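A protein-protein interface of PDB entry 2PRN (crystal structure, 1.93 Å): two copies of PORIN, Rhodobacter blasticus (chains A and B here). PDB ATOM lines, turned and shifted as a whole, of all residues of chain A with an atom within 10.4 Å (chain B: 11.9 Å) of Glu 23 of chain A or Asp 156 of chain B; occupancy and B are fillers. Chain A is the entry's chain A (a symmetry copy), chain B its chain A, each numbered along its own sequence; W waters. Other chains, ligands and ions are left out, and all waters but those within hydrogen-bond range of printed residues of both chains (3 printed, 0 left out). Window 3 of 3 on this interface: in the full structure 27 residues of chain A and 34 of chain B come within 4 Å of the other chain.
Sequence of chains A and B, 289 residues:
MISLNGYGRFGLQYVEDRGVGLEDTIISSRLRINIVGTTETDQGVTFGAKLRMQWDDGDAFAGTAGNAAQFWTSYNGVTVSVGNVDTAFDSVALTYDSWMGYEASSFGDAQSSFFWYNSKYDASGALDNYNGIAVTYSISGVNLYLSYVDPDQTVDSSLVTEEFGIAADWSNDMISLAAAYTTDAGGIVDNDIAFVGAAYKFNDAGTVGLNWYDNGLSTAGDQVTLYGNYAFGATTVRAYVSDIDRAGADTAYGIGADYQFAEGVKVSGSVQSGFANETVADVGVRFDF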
ATOM      1  N   LEU A  12     -31.979 -12.066  25.591  1.00  0.00           N
ATOM      2  CA  LEU A  12     -31.385 -12.941  24.590  1.00  0.00           C
ATOM      3  C   LEU A  12     -30.476 -12.091  23.691  1.00  0.00           C
ATOM      4  O   LEU A  12     -30.783 -10.942  23.353  1.00  0.00           O
ATOM      5  CB  LEU A  12     -32.460 -13.650  23.751  1.00  0.00           C
ATOM      6  CG  LEU A  12     -33.405 -14.560  24.586  1.00  0.00           C
ATOM      7  CD1 LEU A  12     -34.613 -14.941  23.743  1.00  0.00           C
ATOM      8  CD2 LEU A  12     -32.650 -15.791  25.060  1.00  0.00           C
ATOM      9  N   GLN A  13     -29.348 -12.683  23.371  1.00  0.00           N
ATOM     10  CA  GLN A  13     -28.335 -12.065  22.517  1.00  0.00           C
ATOM     11  C   GLN A  13     -27.987 -13.082  21.399  1.00  0.00           C
ATOM     12  O   GLN A  13     -27.505 -14.177  21.687  1.00  0.00           O
ATOM     13  CB  GLN A  13     -27.069 -11.704  23.267  1.00  0.00           C
ATOM     14  CG  GLN A  13     -26.055 -10.952  22.412  1.00  0.00           C
ATOM     15  CD  GLN A  13     -24.660 -11.136  22.979  1.00  0.00           C
ATOM     16  OE1 GLN A  13     -24.011 -12.128  22.667  1.00  0.00           O
ATOM     17  NE2 GLN A  13     -24.201 -10.234  23.838  1.00  0.00           N
ATOM     18  N   TYR A  14     -28.314 -12.707  20.185  1.00  0.00           N
ATOM     19  CA  TYR A  14     -28.106 -13.543  19.002  1.00  0.00           C
ATOM     20  C   TYR A  14     -27.023 -12.947  18.106  1.00  0.00           C
ATOM     21  O   TYR A  14     -27.086 -11.752  17.773  1.00  0.00           O
ATOM     22  CB  TYR A  14     -29.425 -13.649  18.226  1.00  0.00           C
ATOM     23  CG  TYR A  14     -29.272 -14.257  16.833  1.00  0.00           C
ATOM     24  CD1 TYR A  14     -29.183 -15.630  16.657  1.00  0.00           C
ATOM     25  CD2 TYR A  14     -29.205 -13.449  15.720  1.00  0.00           C
ATOM     26  CE1 TYR A  14     -29.054 -16.190  15.391  1.00  0.00           C
ATOM     27  CE2 TYR A  14     -29.075 -13.975  14.453  1.00  0.00           C
ATOM     28  CZ  TYR A  14     -29.008 -15.355  14.299  1.00  0.00           C
ATOM     29  OH  TYR A  14     -28.858 -15.844  13.025  1.00  0.00           O
ATOM     30  N   VAL A  15     -26.053 -13.764  17.726  1.00  0.00           N
ATOM     31  CA  VAL A  15     -24.959 -13.364  16.850  1.00  0.00           C
ATOM     32  C   VAL A  15     -24.920 -14.419  15.723  1.00  0.00           C
ATOM     33  O   VAL A  15     -24.609 -15.586  16.018  1.00  0.00           O
ATOM     34  CB  VAL A  15     -23.584 -13.264  17.498  1.00  0.00           C
ATOM     35  CG1 VAL A  15     -22.561 -12.853  16.417  1.00  0.00           C
ATOM     36  CG2 VAL A  15     -23.564 -12.212  18.600  1.00  0.00           C
ATOM     37  N   GLU A  16     -25.352 -14.059  14.519  1.00  0.00           N
ATOM     38  CA  GLU A  16     -25.394 -15.048  13.434  1.00  0.00           C
ATOM     39  C   GLU A  16     -24.026 -15.700  13.216  1.00  0.00           C
ATOM     40  O   GLU A  16     -23.057 -14.965  13.028  1.00  0.00           O
ATOM     41  CB  GLU A  16     -25.819 -14.396  12.118  1.00  0.00           C
ATOM     42  CG  GLU A  16     -26.280 -15.454  11.099  1.00  0.00           C
ATOM     43  CD  GLU A  16     -26.767 -14.837   9.793  1.00  0.00           C
ATOM     44  OE1 GLU A  16     -26.280 -13.742   9.412  1.00  0.00           O
ATOM     45  OE2 GLU A  16     -27.634 -15.458   9.143  1.00  0.00           O
ATOM     46  N   ASP A  17     -23.963 -17.026  13.248  1.00  0.00           N
ATOM     47  CA  ASP A  17     -22.752 -17.795  13.077  1.00  0.00           C
ATOM     48  C   ASP A  17     -21.601 -17.351  13.981  1.00  0.00           C
ATOM     49  O   ASP A  17     -20.479 -17.105  13.515  1.00  0.00           O
ATOM     50  CB  ASP A  17     -22.214 -17.809  11.648  1.00  0.00           C
ATOM     51  CG  ASP A  17     -23.212 -18.261  10.621  1.00  0.00           C
ATOM     52  OD1 ASP A  17     -23.978 -19.216  10.882  1.00  0.00           O
ATOM     53  OD2 ASP A  17     -23.237 -17.639   9.522  1.00  0.00           O
ATOM     54  N   ARG A  18     -21.835 -17.312  15.271  1.00  0.00           N
ATOM     55  CA  ARG A  18     -20.878 -16.884  16.269  1.00  0.00           C
ATOM     56  C   ARG A  18     -19.581 -17.659  16.210  1.00  0.00           C
ATOM     57  O   ARG A  18     -18.503 -17.091  16.450  1.00  0.00           O
ATOM     58  CB  ARG A  18     -21.554 -17.054  17.636  1.00  0.00           C
ATOM     59  CG  ARG A  18     -20.939 -16.370  18.815  1.00  0.00           C
ATOM     60  CD  ARG A  18     -21.651 -16.788  20.087  1.00  0.00           C
ATOM     61  NE  ARG A  18     -22.967 -16.189  20.272  1.00  0.00           N
ATOM     62  CZ  ARG A  18     -23.217 -15.036  20.893  1.00  0.00           C
ATOM     63  NH1 ARG A  18     -22.248 -14.263  21.381  1.00  0.00           N
ATOM     64  NH2 ARG A  18     -24.472 -14.641  21.045  1.00  0.00           N
ATOM     65  N   GLY A  19     -19.629 -18.965  15.914  1.00  0.00           N
ATOM     66  CA  GLY A  19     -18.335 -19.695  15.910  1.00  0.00           C
ATOM     67  C   GLY A  19     -18.600 -21.192  15.821  1.00  0.00           C
ATOM     68  O   GLY A  19     -19.700 -21.671  16.140  1.00  0.00           O
ATOM     69  N   VAL A  20     -17.568 -21.904  15.371  1.00  0.00           N
ATOM     70  CA  VAL A  20     -17.713 -23.352  15.208  1.00  0.00           C
ATOM     71  C   VAL A  20     -17.883 -24.008  16.550  1.00  0.00           C
ATOM     72  O   VAL A  20     -17.087 -23.793  17.456  1.00  0.00           O
ATOM     73  CB  VAL A  20     -16.639 -23.931  14.287  1.00  0.00           C
ATOM     74  CG1 VAL A  20     -15.437 -24.509  15.001  1.00  0.00           C
ATOM     75  CG2 VAL A  20     -17.303 -24.998  13.396  1.00  0.00           C
ATOM     76  N   GLY A  21     -18.986 -24.727  16.722  1.00  0.00           N
ATOM     77  CA  GLY A  21     -19.263 -25.371  17.991  1.00  0.00           C
ATOM     78  C   GLY A  21     -19.890 -24.455  19.029  1.00  0.00           C
ATOM     79  O   GLY A  21     -20.049 -24.877  20.186  1.00  0.00           O
ATOM     80  N   LEU A  22     -20.258 -23.243  18.659  1.00  0.00           N
ATOM     81  CA  LEU A  22     -20.844 -22.278  19.567  1.00  0.00           C
ATOM     82  C   LEU A  22     -22.328 -22.073  19.287  1.00  0.00           C
ATOM     83  O   LEU A  22     -22.821 -22.227  18.183  1.00  0.00           O
ATOM     84  CB  LEU A  22     -20.172 -20.917  19.505  1.00  0.00           C
ATOM     85  CG  LEU A  22     -18.690 -20.814  19.820  1.00  0.00           C
ATOM     86  CD1 LEU A  22     -18.227 -19.373  19.600  1.00  0.00           C
ATOM     87  CD2 LEU A  22     -18.391 -21.262  21.231  1.00  0.00           C
ATOM     88  N   GLU A  23     -23.028 -21.736  20.343  1.00  0.00           N
ATOM     89  CA  GLU A  23     -24.460 -21.449  20.272  1.00  0.00           C
ATOM     90  C   GLU A  23     -24.604 -20.020  19.776  1.00  0.00           C
ATOM     91  O   GLU A  23     -23.928 -19.120  20.280  1.00  0.00           O
ATOM     92  CB  GLU A  23     -25.007 -21.623  21.691  1.00  0.00           C
ATOM     93  CG  GLU A  23     -26.438 -21.934  21.886  1.00  0.00           C
ATOM     94  CD  GLU A  23     -26.976 -23.118  21.100  1.00  0.00           C
ATOM     95  OE1 GLU A  23     -26.776 -24.272  21.494  1.00  0.00           O
ATOM     96  OE2 GLU A  23     -27.614 -22.823  20.065  1.00  0.00           O
ATOM     97  N   ASP A  24     -25.454 -19.766  18.784  1.00  0.00           N
ATOM     98  CA  ASP A  24     -25.616 -18.425  18.275  1.00  0.00           C
ATOM     99  C   ASP A  24     -26.380 -17.490  19.235  1.00  0.00           C
ATOM    100  O   ASP A  24     -26.095 -16.289  19.257  1.00  0.00           O
ATOM    101  CB  ASP A  24     -26.455 -18.445  16.984  1.00  0.00           C
ATOM    102  CG  ASP A  24     -25.594 -18.737  15.757  1.00  0.00           C
ATOM    103  OD1 ASP A  24     -24.355 -18.791  15.856  1.00  0.00           O
ATOM    104  OD2 ASP A  24     -26.226 -18.928  14.699  1.00  0.00           O
ATOM    105  N   THR A  25     -27.320 -18.079  19.929  1.00  0.00           N
ATOM    106  CA  THR A  25     -28.158 -17.380  20.870  1.00  0.00           C
ATOM    107  C   THR A  25     -27.763 -17.712  22.309  1.00  0.00           C
ATOM    108  O   THR A  25     -27.587 -18.885  22.642  1.00  0.00           O
ATOM    109  CB  THR A  25     -29.639 -17.694  20.633  1.00  0.00           C
ATOM    110  OG1 THR A  25     -30.015 -17.247  19.305  1.00  0.00           O
ATOM    111  CG2 THR A  25     -30.529 -16.962  21.630  1.00  0.00           C
ATOM    112  N   ILE A  26     -27.476 -16.693  23.113  1.00  0.00           N
ATOM    113  CA  ILE A  26     -27.198 -16.936  24.527  1.00  0.00           C
ATOM    114  C   ILE A  26     -28.022 -16.011  25.446  1.00  0.00           C
ATOM    115  O   ILE A  26     -28.639 -15.052  24.987  1.00  0.00           O
ATOM    116  CB  ILE A  26     -25.711 -16.749  24.899  1.00  0.00           C
ATOM    117  CG1 ILE A  26     -25.311 -15.269  24.738  1.00  0.00           C
ATOM    118  CG2 ILE A  26     -24.835 -17.663  24.090  1.00  0.00           C
ATOM    119  CD1 ILE A  26     -23.926 -14.984  25.306  1.00  0.00           C
ATOM    120  N   ILE A  27     -28.032 -16.356  26.732  1.00  0.00           N
ATOM    121  CA  ILE A  27     -28.690 -15.463  27.705  1.00  0.00           C
ATOM    122  C   ILE A  27     -27.622 -14.506  28.213  1.00  0.00           C
ATOM    123  O   ILE A  27     -26.661 -14.872  28.934  1.00  0.00           O
ATOM    124  CB  ILE A  27     -29.444 -16.132  28.818  1.00  0.00           C
ATOM    125  CG1 ILE A  27     -30.714 -16.831  28.245  1.00  0.00           C
ATOM    126  CG2 ILE A  27     -29.865 -15.177  29.926  1.00  0.00           C
ATOM    127  CD1 ILE A  27     -31.212 -17.915  29.187  1.00  0.00           C
ATOM    128  N   SER A  28     -27.750 -13.273  27.812  1.00  0.00           N
ATOM    129  CA  SER A  28     -26.752 -12.274  28.184  1.00  0.00           C
ATOM    130  C   SER A  28     -27.282 -11.360  29.289  1.00  0.00           C
ATOM    131  O   SER A  28     -28.382 -10.820  29.131  1.00  0.00           O
ATOM    132  CB  SER A  28     -26.393 -11.421  26.967  1.00  0.00           C
ATOM    133  OG  SER A  28     -25.611 -10.331  27.419  1.00  0.00           O
ATOM    134  N   ASP A  57     -22.212 -11.778  32.155  1.00  0.00           N
ATOM    135  CA  ASP A  57     -22.187 -13.230  31.855  1.00  0.00           C
ATOM    136  C   ASP A  57     -20.862 -13.517  31.132  1.00  0.00           C
ATOM    137  O   ASP A  57     -20.406 -12.708  30.327  1.00  0.00           O
ATOM    138  CB  ASP A  57     -23.398 -13.658  31.028  1.00  0.00           C
ATOM    139  CG  ASP A  57     -23.362 -13.019  29.654  1.00  0.00           C
ATOM    140  OD1 ASP A  57     -23.830 -11.868  29.587  1.00  0.00           O
ATOM    141  OD2 ASP A  57     -22.839 -13.570  28.668  1.00  0.00           O
ATOM    142  N   THR A 279     -24.540 -10.078  11.602  1.00  0.00           N
ATOM    143  CA  THR A 279     -25.927  -9.919  11.954  1.00  0.00           C
ATOM    144  C   THR A 279     -26.105 -10.204  13.448  1.00  0.00           C
ATOM    145  O   THR A 279     -25.709 -11.217  14.018  1.00  0.00           O
ATOM    146  CB  THR A 279     -26.861 -10.794  11.100  1.00  0.00           C
ATOM    147  OG1 THR A 279     -26.653 -10.341   9.749  1.00  0.00           O
ATOM    148  CG2 THR A 279     -28.315 -10.486  11.471  1.00  0.00           C
ATOM    149  N   ASN B 129     -19.308 -19.778  32.210  1.00  0.00           N
ATOM    150  CA  ASN B 129     -20.454 -19.613  31.310  1.00  0.00           C
ATOM    151  C   ASN B 129     -21.643 -20.407  31.786  1.00  0.00           C
ATOM    152  O   ASN B 129     -22.519 -20.768  31.010  1.00  0.00           O
ATOM    153  CB  ASN B 129     -20.027 -20.098  29.903  1.00  0.00           C
ATOM    154  CG  ASN B 129     -19.069 -19.064  29.315  1.00  0.00           C
ATOM    155  OD1 ASN B 129     -19.493 -17.958  28.986  1.00  0.00           O
ATOM    156  ND2 ASN B 129     -17.793 -19.364  29.226  1.00  0.00           N
ATOM    157  N   ASN B 131     -25.101 -21.058  33.400  1.00  0.00           N
ATOM    158  CA  ASN B 131     -26.336 -20.277  33.426  1.00  0.00           C
ATOM    159  C   ASN B 131     -27.544 -21.150  33.675  1.00  0.00           C
ATOM    160  O   ASN B 131     -27.674 -22.228  33.095  1.00  0.00           O
ATOM    161  CB  ASN B 131     -26.437 -19.501  32.114  1.00  0.00           C
ATOM    162  CG  ASN B 131     -27.495 -18.433  32.193  1.00  0.00           C
ATOM    163  OD1 ASN B 131     -27.241 -17.395  32.800  1.00  0.00           O
ATOM    164  ND2 ASN B 131     -28.656 -18.669  31.615  1.00  0.00           N
ATOM    165  N   TYR B 148     -33.480 -25.611  35.387  1.00  0.00           N
ATOM    166  CA  TYR B 148     -32.691 -26.054  34.238  1.00  0.00           C
ATOM    167  C   TYR B 148     -31.338 -25.364  34.294  1.00  0.00           C
ATOM    168  O   TYR B 148     -31.268 -24.114  34.369  1.00  0.00           O
ATOM    169  CB  TYR B 148     -33.427 -25.670  32.937  1.00  0.00           C
ATOM    170  CG  TYR B 148     -32.588 -25.855  31.698  1.00  0.00           C
ATOM    171  CD1 TYR B 148     -32.412 -27.111  31.119  1.00  0.00           C
ATOM    172  CD2 TYR B 148     -31.969 -24.747  31.128  1.00  0.00           C
ATOM    173  CE1 TYR B 148     -31.625 -27.236  29.970  1.00  0.00           C
ATOM    174  CE2 TYR B 148     -31.185 -24.858  30.000  1.00  0.00           C
ATOM    175  CZ  TYR B 148     -31.022 -26.120  29.438  1.00  0.00           C
ATOM    176  OH  TYR B 148     -30.196 -26.224  28.332  1.00  0.00           O
ATOM    177  N   VAL B 149     -30.266 -26.124  34.382  1.00  0.00           N
ATOM    178  CA  VAL B 149     -28.938 -25.498  34.480  1.00  0.00           C
ATOM    179  C   VAL B 149     -28.071 -25.936  33.322  1.00  0.00           C
ATOM    180  O   VAL B 149     -27.934 -27.144  33.049  1.00  0.00           O
ATOM    181  CB  VAL B 149     -28.252 -25.853  35.816  1.00  0.00           C
ATOM    182  CG1 VAL B 149     -26.836 -25.318  35.879  1.00  0.00           C
ATOM    183  CG2 VAL B 149     -29.073 -25.318  36.987  1.00  0.00           C
ATOM    184  N   ASP B 150     -27.518 -24.970  32.616  1.00  0.00           N
ATOM    185  CA  ASP B 150     -26.585 -25.294  31.515  1.00  0.00           C
ATOM    186  C   ASP B 150     -25.217 -24.874  32.019  1.00  0.00           C
ATOM    187  O   ASP B 150     -24.962 -23.672  32.213  1.00  0.00           O
ATOM    188  CB  ASP B 150     -27.055 -24.618  30.260  1.00  0.00           C
ATOM    189  CG  ASP B 150     -26.140 -24.918  29.078  1.00  0.00           C
ATOM    190  OD1 ASP B 150     -25.060 -25.484  29.292  1.00  0.00           O
ATOM    191  OD2 ASP B 150     -26.530 -24.561  27.950  1.00  0.00           O
ATOM    192  N   PRO B 151     -24.307 -25.807  32.267  1.00  0.00           N
ATOM    193  CA  PRO B 151     -22.997 -25.504  32.790  1.00  0.00           C
ATOM    194  C   PRO B 151     -22.080 -24.685  31.905  1.00  0.00           C
ATOM    195  O   PRO B 151     -21.087 -24.103  32.388  1.00  0.00           O
ATOM    196  CB  PRO B 151     -22.390 -26.848  33.116  1.00  0.00           C
ATOM    197  CG  PRO B 151     -23.239 -27.885  32.488  1.00  0.00           C
ATOM    198  CD  PRO B 151     -24.522 -27.253  32.048  1.00  0.00           C
ATOM    199  N   ASP B 152     -22.327 -24.603  30.620  1.00  0.00           N
ATOM    200  CA  ASP B 152     -21.538 -23.822  29.688  1.00  0.00           C
ATOM    201  C   ASP B 152     -22.501 -23.461  28.553  1.00  0.00           C
ATOM    202  O   ASP B 152     -22.606 -24.182  27.535  1.00  0.00           O
ATOM    203  CB  ASP B 152     -20.309 -24.538  29.133  1.00  0.00           C
ATOM    204  CG  ASP B 152     -19.390 -23.613  28.354  1.00  0.00           C
ATOM    205  OD1 ASP B 152     -19.816 -22.607  27.737  1.00  0.00           O
ATOM    206  OD2 ASP B 152     -18.170 -23.901  28.301  1.00  0.00           O
ATOM    207  N   GLN B 153     -23.219 -22.351  28.746  1.00  0.00           N
ATOM    208  CA  GLN B 153     -24.209 -21.941  27.775  1.00  0.00           C
ATOM    209  C   GLN B 153     -23.646 -21.441  26.472  1.00  0.00           C
ATOM    210  O   GLN B 153     -24.446 -21.295  25.532  1.00  0.00           O
ATOM    211  CB  GLN B 153     -25.168 -20.877  28.403  1.00  0.00           C
ATOM    212  CG  GLN B 153     -24.470 -19.504  28.489  1.00  0.00           C
ATOM    213  CD  GLN B 153     -25.438 -18.352  28.525  1.00  0.00           C
ATOM    214  OE1 GLN B 153     -26.595 -18.485  28.113  1.00  0.00           O
ATOM    215  NE2 GLN B 153     -24.991 -17.176  28.991  1.00  0.00           N
ATOM    216  N   THR B 154     -22.365 -21.182  26.283  1.00  0.00           N
ATOM    217  CA  THR B 154     -21.871 -20.666  25.027  1.00  0.00           C
ATOM    218  C   THR B 154     -21.683 -21.812  24.015  1.00  0.00           C
ATOM    219  O   THR B 154     -21.700 -21.591  22.803  1.00  0.00           O
ATOM    220  CB  THR B 154     -20.546 -19.891  25.155  1.00  0.00           C
ATOM    221  OG1 THR B 154     -19.577 -20.861  25.620  1.00  0.00           O
ATOM    222  CG2 THR B 154     -20.572 -18.768  26.183  1.00  0.00           C
ATOM    223  N   VAL B 155     -21.462 -23.016  24.520  1.00  0.00           N
ATOM    224  CA  VAL B 155     -21.218 -24.174  23.651  1.00  0.00           C
ATOM    225  C   VAL B 155     -22.507 -24.811  23.206  1.00  0.00           C
ATOM    226  O   VAL B 155     -23.535 -24.844  23.910  1.00  0.00           O
ATOM    227  CB  VAL B 155     -20.306 -25.175  24.397  1.00  0.00           C
ATOM    228  CG1 VAL B 155     -20.201 -26.471  23.639  1.00  0.00           C
ATOM    229  CG2 VAL B 155     -18.926 -24.539  24.599  1.00  0.00           C
ATOM    230  N   ASP B 156     -22.527 -25.333  21.979  1.00  0.00           N
ATOM    231  CA  ASP B 156     -23.737 -25.981  21.456  1.00  0.00           C
ATOM    232  C   ASP B 156     -24.389 -26.896  22.479  1.00  0.00           C
ATOM    233  O   ASP B 156     -23.701 -27.780  23.018  1.00  0.00           O
ATOM    234  CB  ASP B 156     -23.243 -26.814  20.249  1.00  0.00           C
ATOM    235  CG  ASP B 156     -24.436 -27.237  19.413  1.00  0.00           C
ATOM    236  OD1 ASP B 156     -25.220 -28.111  19.864  1.00  0.00           O
ATOM    237  OD2 ASP B 156     -24.549 -26.629  18.317  1.00  0.00           O
ATOM    238  N   SER B 157     -25.708 -26.836  22.706  1.00  0.00           N
ATOM    239  CA  SER B 157     -26.329 -27.643  23.719  1.00  0.00           C
ATOM    240  C   SER B 157     -26.122 -29.147  23.634  1.00  0.00           C
ATOM    241  O   SER B 157     -26.153 -29.789  24.711  1.00  0.00           O
ATOM    242  CB  SER B 157     -27.838 -27.437  23.895  1.00  0.00           C
ATOM    243  OG  SER B 157     -28.335 -26.593  22.890  1.00  0.00           O
ATOM    244  N   SER B 158     -25.986 -29.730  22.464  1.00  0.00           N
ATOM    245  CA  SER B 158     -25.828 -31.184  22.371  1.00  0.00           C
ATOM    246  C   SER B 158     -24.451 -31.647  22.810  1.00  0.00           C
ATOM    247  O   SER B 158     -24.224 -32.876  22.955  1.00  0.00           O
ATOM    248  CB  SER B 158     -26.049 -31.592  20.896  1.00  0.00           C
ATOM    249  OG  SER B 158     -24.807 -31.283  20.217  1.00  0.00           O
ATOM    250  N   LEU B 159     -23.509 -30.734  23.016  1.00  0.00           N
ATOM    251  CA  LEU B 159     -22.174 -31.119  23.434  1.00  0.00           C
ATOM    252  C   LEU B 159     -21.970 -31.085  24.937  1.00  0.00           C
ATOM    253  O   LEU B 159     -20.878 -31.412  25.436  1.00  0.00           O
ATOM    254  CB  LEU B 159     -21.162 -30.148  22.792  1.00  0.00           C
ATOM    255  CG  LEU B 159     -21.010 -30.307  21.271  1.00  0.00           C
ATOM    256  CD1 LEU B 159     -20.294 -29.116  20.680  1.00  0.00           C
ATOM    257  CD2 LEU B 159     -20.273 -31.599  20.927  1.00  0.00           C
ATOM    258  N   VAL B 160     -22.934 -30.568  25.699  1.00  0.00           N
ATOM    259  CA  VAL B 160     -22.755 -30.461  27.156  1.00  0.00           C
ATOM    260  C   VAL B 160     -23.973 -31.101  27.823  1.00  0.00           C
ATOM    261  O   VAL B 160     -25.033 -31.216  27.191  1.00  0.00           O
ATOM    262  CB  VAL B 160     -22.580 -29.020  27.657  1.00  0.00           C
ATOM    263  CG1 VAL B 160     -21.677 -28.186  26.751  1.00  0.00           C
ATOM    264  CG2 VAL B 160     -23.910 -28.297  27.771  1.00  0.00           C
ATOM    265  N   THR B 161     -23.845 -31.491  29.055  1.00  0.00           N
ATOM    266  CA  THR B 161     -24.951 -32.114  29.778  1.00  0.00           C
ATOM    267  C   THR B 161     -25.654 -31.099  30.657  1.00  0.00           C
ATOM    268  O   THR B 161     -24.999 -30.505  31.492  1.00  0.00           O
ATOM    269  CB  THR B 161     -24.385 -33.219  30.712  1.00  0.00           C
ATOM    270  OG1 THR B 161     -23.552 -34.062  29.904  1.00  0.00           O
ATOM    271  CG2 THR B 161     -25.458 -34.013  31.416  1.00  0.00           C
ATOM    272  N   GLU B 162     -26.940 -30.920  30.488  1.00  0.00           N
ATOM    273  CA  GLU B 162     -27.693 -29.983  31.296  1.00  0.00           C
ATOM    274  C   GLU B 162     -28.445 -30.724  32.396  1.00  0.00           C
ATOM    275  O   GLU B 162     -28.897 -31.844  32.206  1.00  0.00           O
ATOM    276  CB  GLU B 162     -28.674 -29.175  30.441  1.00  0.00           C
ATOM    277  CG  GLU B 162     -27.914 -28.282  29.460  1.00  0.00           C
ATOM    278  CD  GLU B 162     -27.711 -28.959  28.120  1.00  0.00           C
ATOM    279  OE1 GLU B 162     -28.364 -29.991  27.836  1.00  0.00           O
ATOM    280  OE2 GLU B 162     -26.859 -28.448  27.350  1.00  0.00           O
ATOM    281  N   GLU B 163     -28.598 -30.053  33.536  1.00  0.00           N
ATOM    282  CA  GLU B 163     -29.323 -30.622  34.652  1.00  0.00           C
ATOM    283  C   GLU B 163     -30.774 -30.188  34.631  1.00  0.00           C
ATOM    284  O   GLU B 163     -31.056 -29.006  34.418  1.00  0.00           O
ATOM    285  CB  GLU B 163     -28.625 -30.230  35.964  1.00  0.00           C
ATOM    286  CG  GLU B 163     -29.390 -30.728  37.172  1.00  0.00           C
ATOM    287  CD  GLU B 163     -28.827 -30.113  38.452  1.00  0.00           C
ATOM    288  OE1 GLU B 163     -27.908 -30.699  39.046  1.00  0.00           O
ATOM    289  OE2 GLU B 163     -29.352 -29.048  38.821  1.00  0.00           O
HETATM  290  O   HOH W   1     -21.888 -19.046  22.200  1.00  0.00           O
HETATM  291  O   HOH W   2     -20.943 -15.039  27.772  1.00  0.00           O
HETATM  292  O   HOH W   3     -26.661 -14.592  31.701  1.00  0.00           O
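The side-chain amide nitrogen (NE2) of Gln 153 of chain B is in hydrogen-bond range of the backbone carbonyl oxygen (O) of Ile 27 of chain A (2.8 Å).
O of Thr 154 of chain B sits at hydrogen-bond distance from N of Glu 23 of chain A (2.8 Å).
The backbone carbonyl oxygen (O) of Gly 21 of chain A is in hydrogen-bond range of the backbone NH (N) of Asp 156 of chain B (3.1 Å).
The side-chain carboxylate (OE1) of Glu 23 of chain A is in hydrogen-bond range of the backbone NH (N) of Ser 157 of chain B (3.0 Å).
The backbone carbonyl oxygen of Asn 129 of chain B is in hydrogen-bond range of the backbone NH of Gln 153 of chain B (2.8 Å).
O of Asn 131 of chain B lies within hydrogen-bond range of N of Asp 150 of chain B, 2.8 Å away.
The side-chain carboxylate of Asp 152 of chain B lies within hydrogen-bond range of the side-chain hydroxyl of Thr 154 of chain B, at 2.8 Å.
OD1 of Asp 156 of chain B is in hydrogen-bond range of N of Ser 158 of chain B (3.2 Å).
O of Gln 13 of chain A is in hydrogen-bond range of N of Ile 26 of chain A.
The backbone carbonyl oxygen of Glu 23 of chain A sits at hydrogen-bond distance from the guanidinium group of Arg 18 of chain A (3.1 Å).
Val 155 of chain B touches Gly 21 of chain A (CA to O, 3.7 Å).
Leu 22 of chain A touches Thr 154 of chain B.
Glu 23 of chain A touches Gln 153 of chain B.
OE1 of Glu 23 of chain A touches CA of Asp 156 of chain B, at 3.5 Å.
CB of Ile 26 of chain A touches OE1 of Gln 153 of chain B, 3.8 Å away.
Asn 131 of chain B touches Ile 27 of chain A.
No residue of chain B comes within 4 Å of Gly 19 of chain A.
Glu 23 of chain A touches just these residues of chain B: Gln 153 (3.9 Å), Thr 154 (2.8 Å), Asp 156 (3.5 Å) and Ser 157 (3.0 Å).
No residue of chain B comes within 4 Å of Asp 24 of chain A.
Printed residues of chain B within 4 Å of Ile 27 of chain A: Asn 131 (3.6 Å) and Gln 153 (2.8 Å).
Printed residues of chain A within 4 Å of Asn 131 of chain B: Ile 27.
Pro 151 of chain B touches none of the printed residues of chain A.
Of the printed residues of chain A, Gln 153 of chain B touches Glu 23 (3.9 Å), Ile 26 (3.8 Å) and Ile 27 (2.8 Å).
Printed residues of chain A within 4 Å of Thr 154 of chain B: Leu 22 and Glu 23.
Of chain A, only Gly 21 and Glu 23 come within 4 Å of Asp 156 of chain B.
Ser 157 of chain B touches one residue of chain A.
Glu 162 of chain B touches none of the printed residues of chain A.
The nearest residue of chain B that does not touch Glu 23 of chain A is Val 155 of chain B (4.1 Å).
The nearest residue of chain A that does not touch Asp 156 of chain B is Leu 22 of chain A (4.2 Å).
Of the 18 printed residues of chain B, 6 touch a printed residue of chain A.
Printed residues of chain A that touch a printed residue of chain B: Gly 21, Leu 22, Glu 23, Ile 26 and Ile 27.
Hydrophobic or aromatic side chains of chain A that line the printed part of chain B: Leu 22, Ile 26 and Ile 27.
Among the printed residues, 10 pairs touch across the chains.
No position is printed for both chains.
Water W2 bridges the side-chain carboxylate (OD2) of Asp 57 of chain A and the side-chain amide oxygen (OD1) of Asn 129 of chain B.
Water W1 bridges O of Thr 154 of chain B and O of Glu 23 of chain A.
Water W3 bridges the backbone carbonyl oxygen of Ile 27 of chain A and the side-chain amide oxygen of Asn 131 of chain B.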
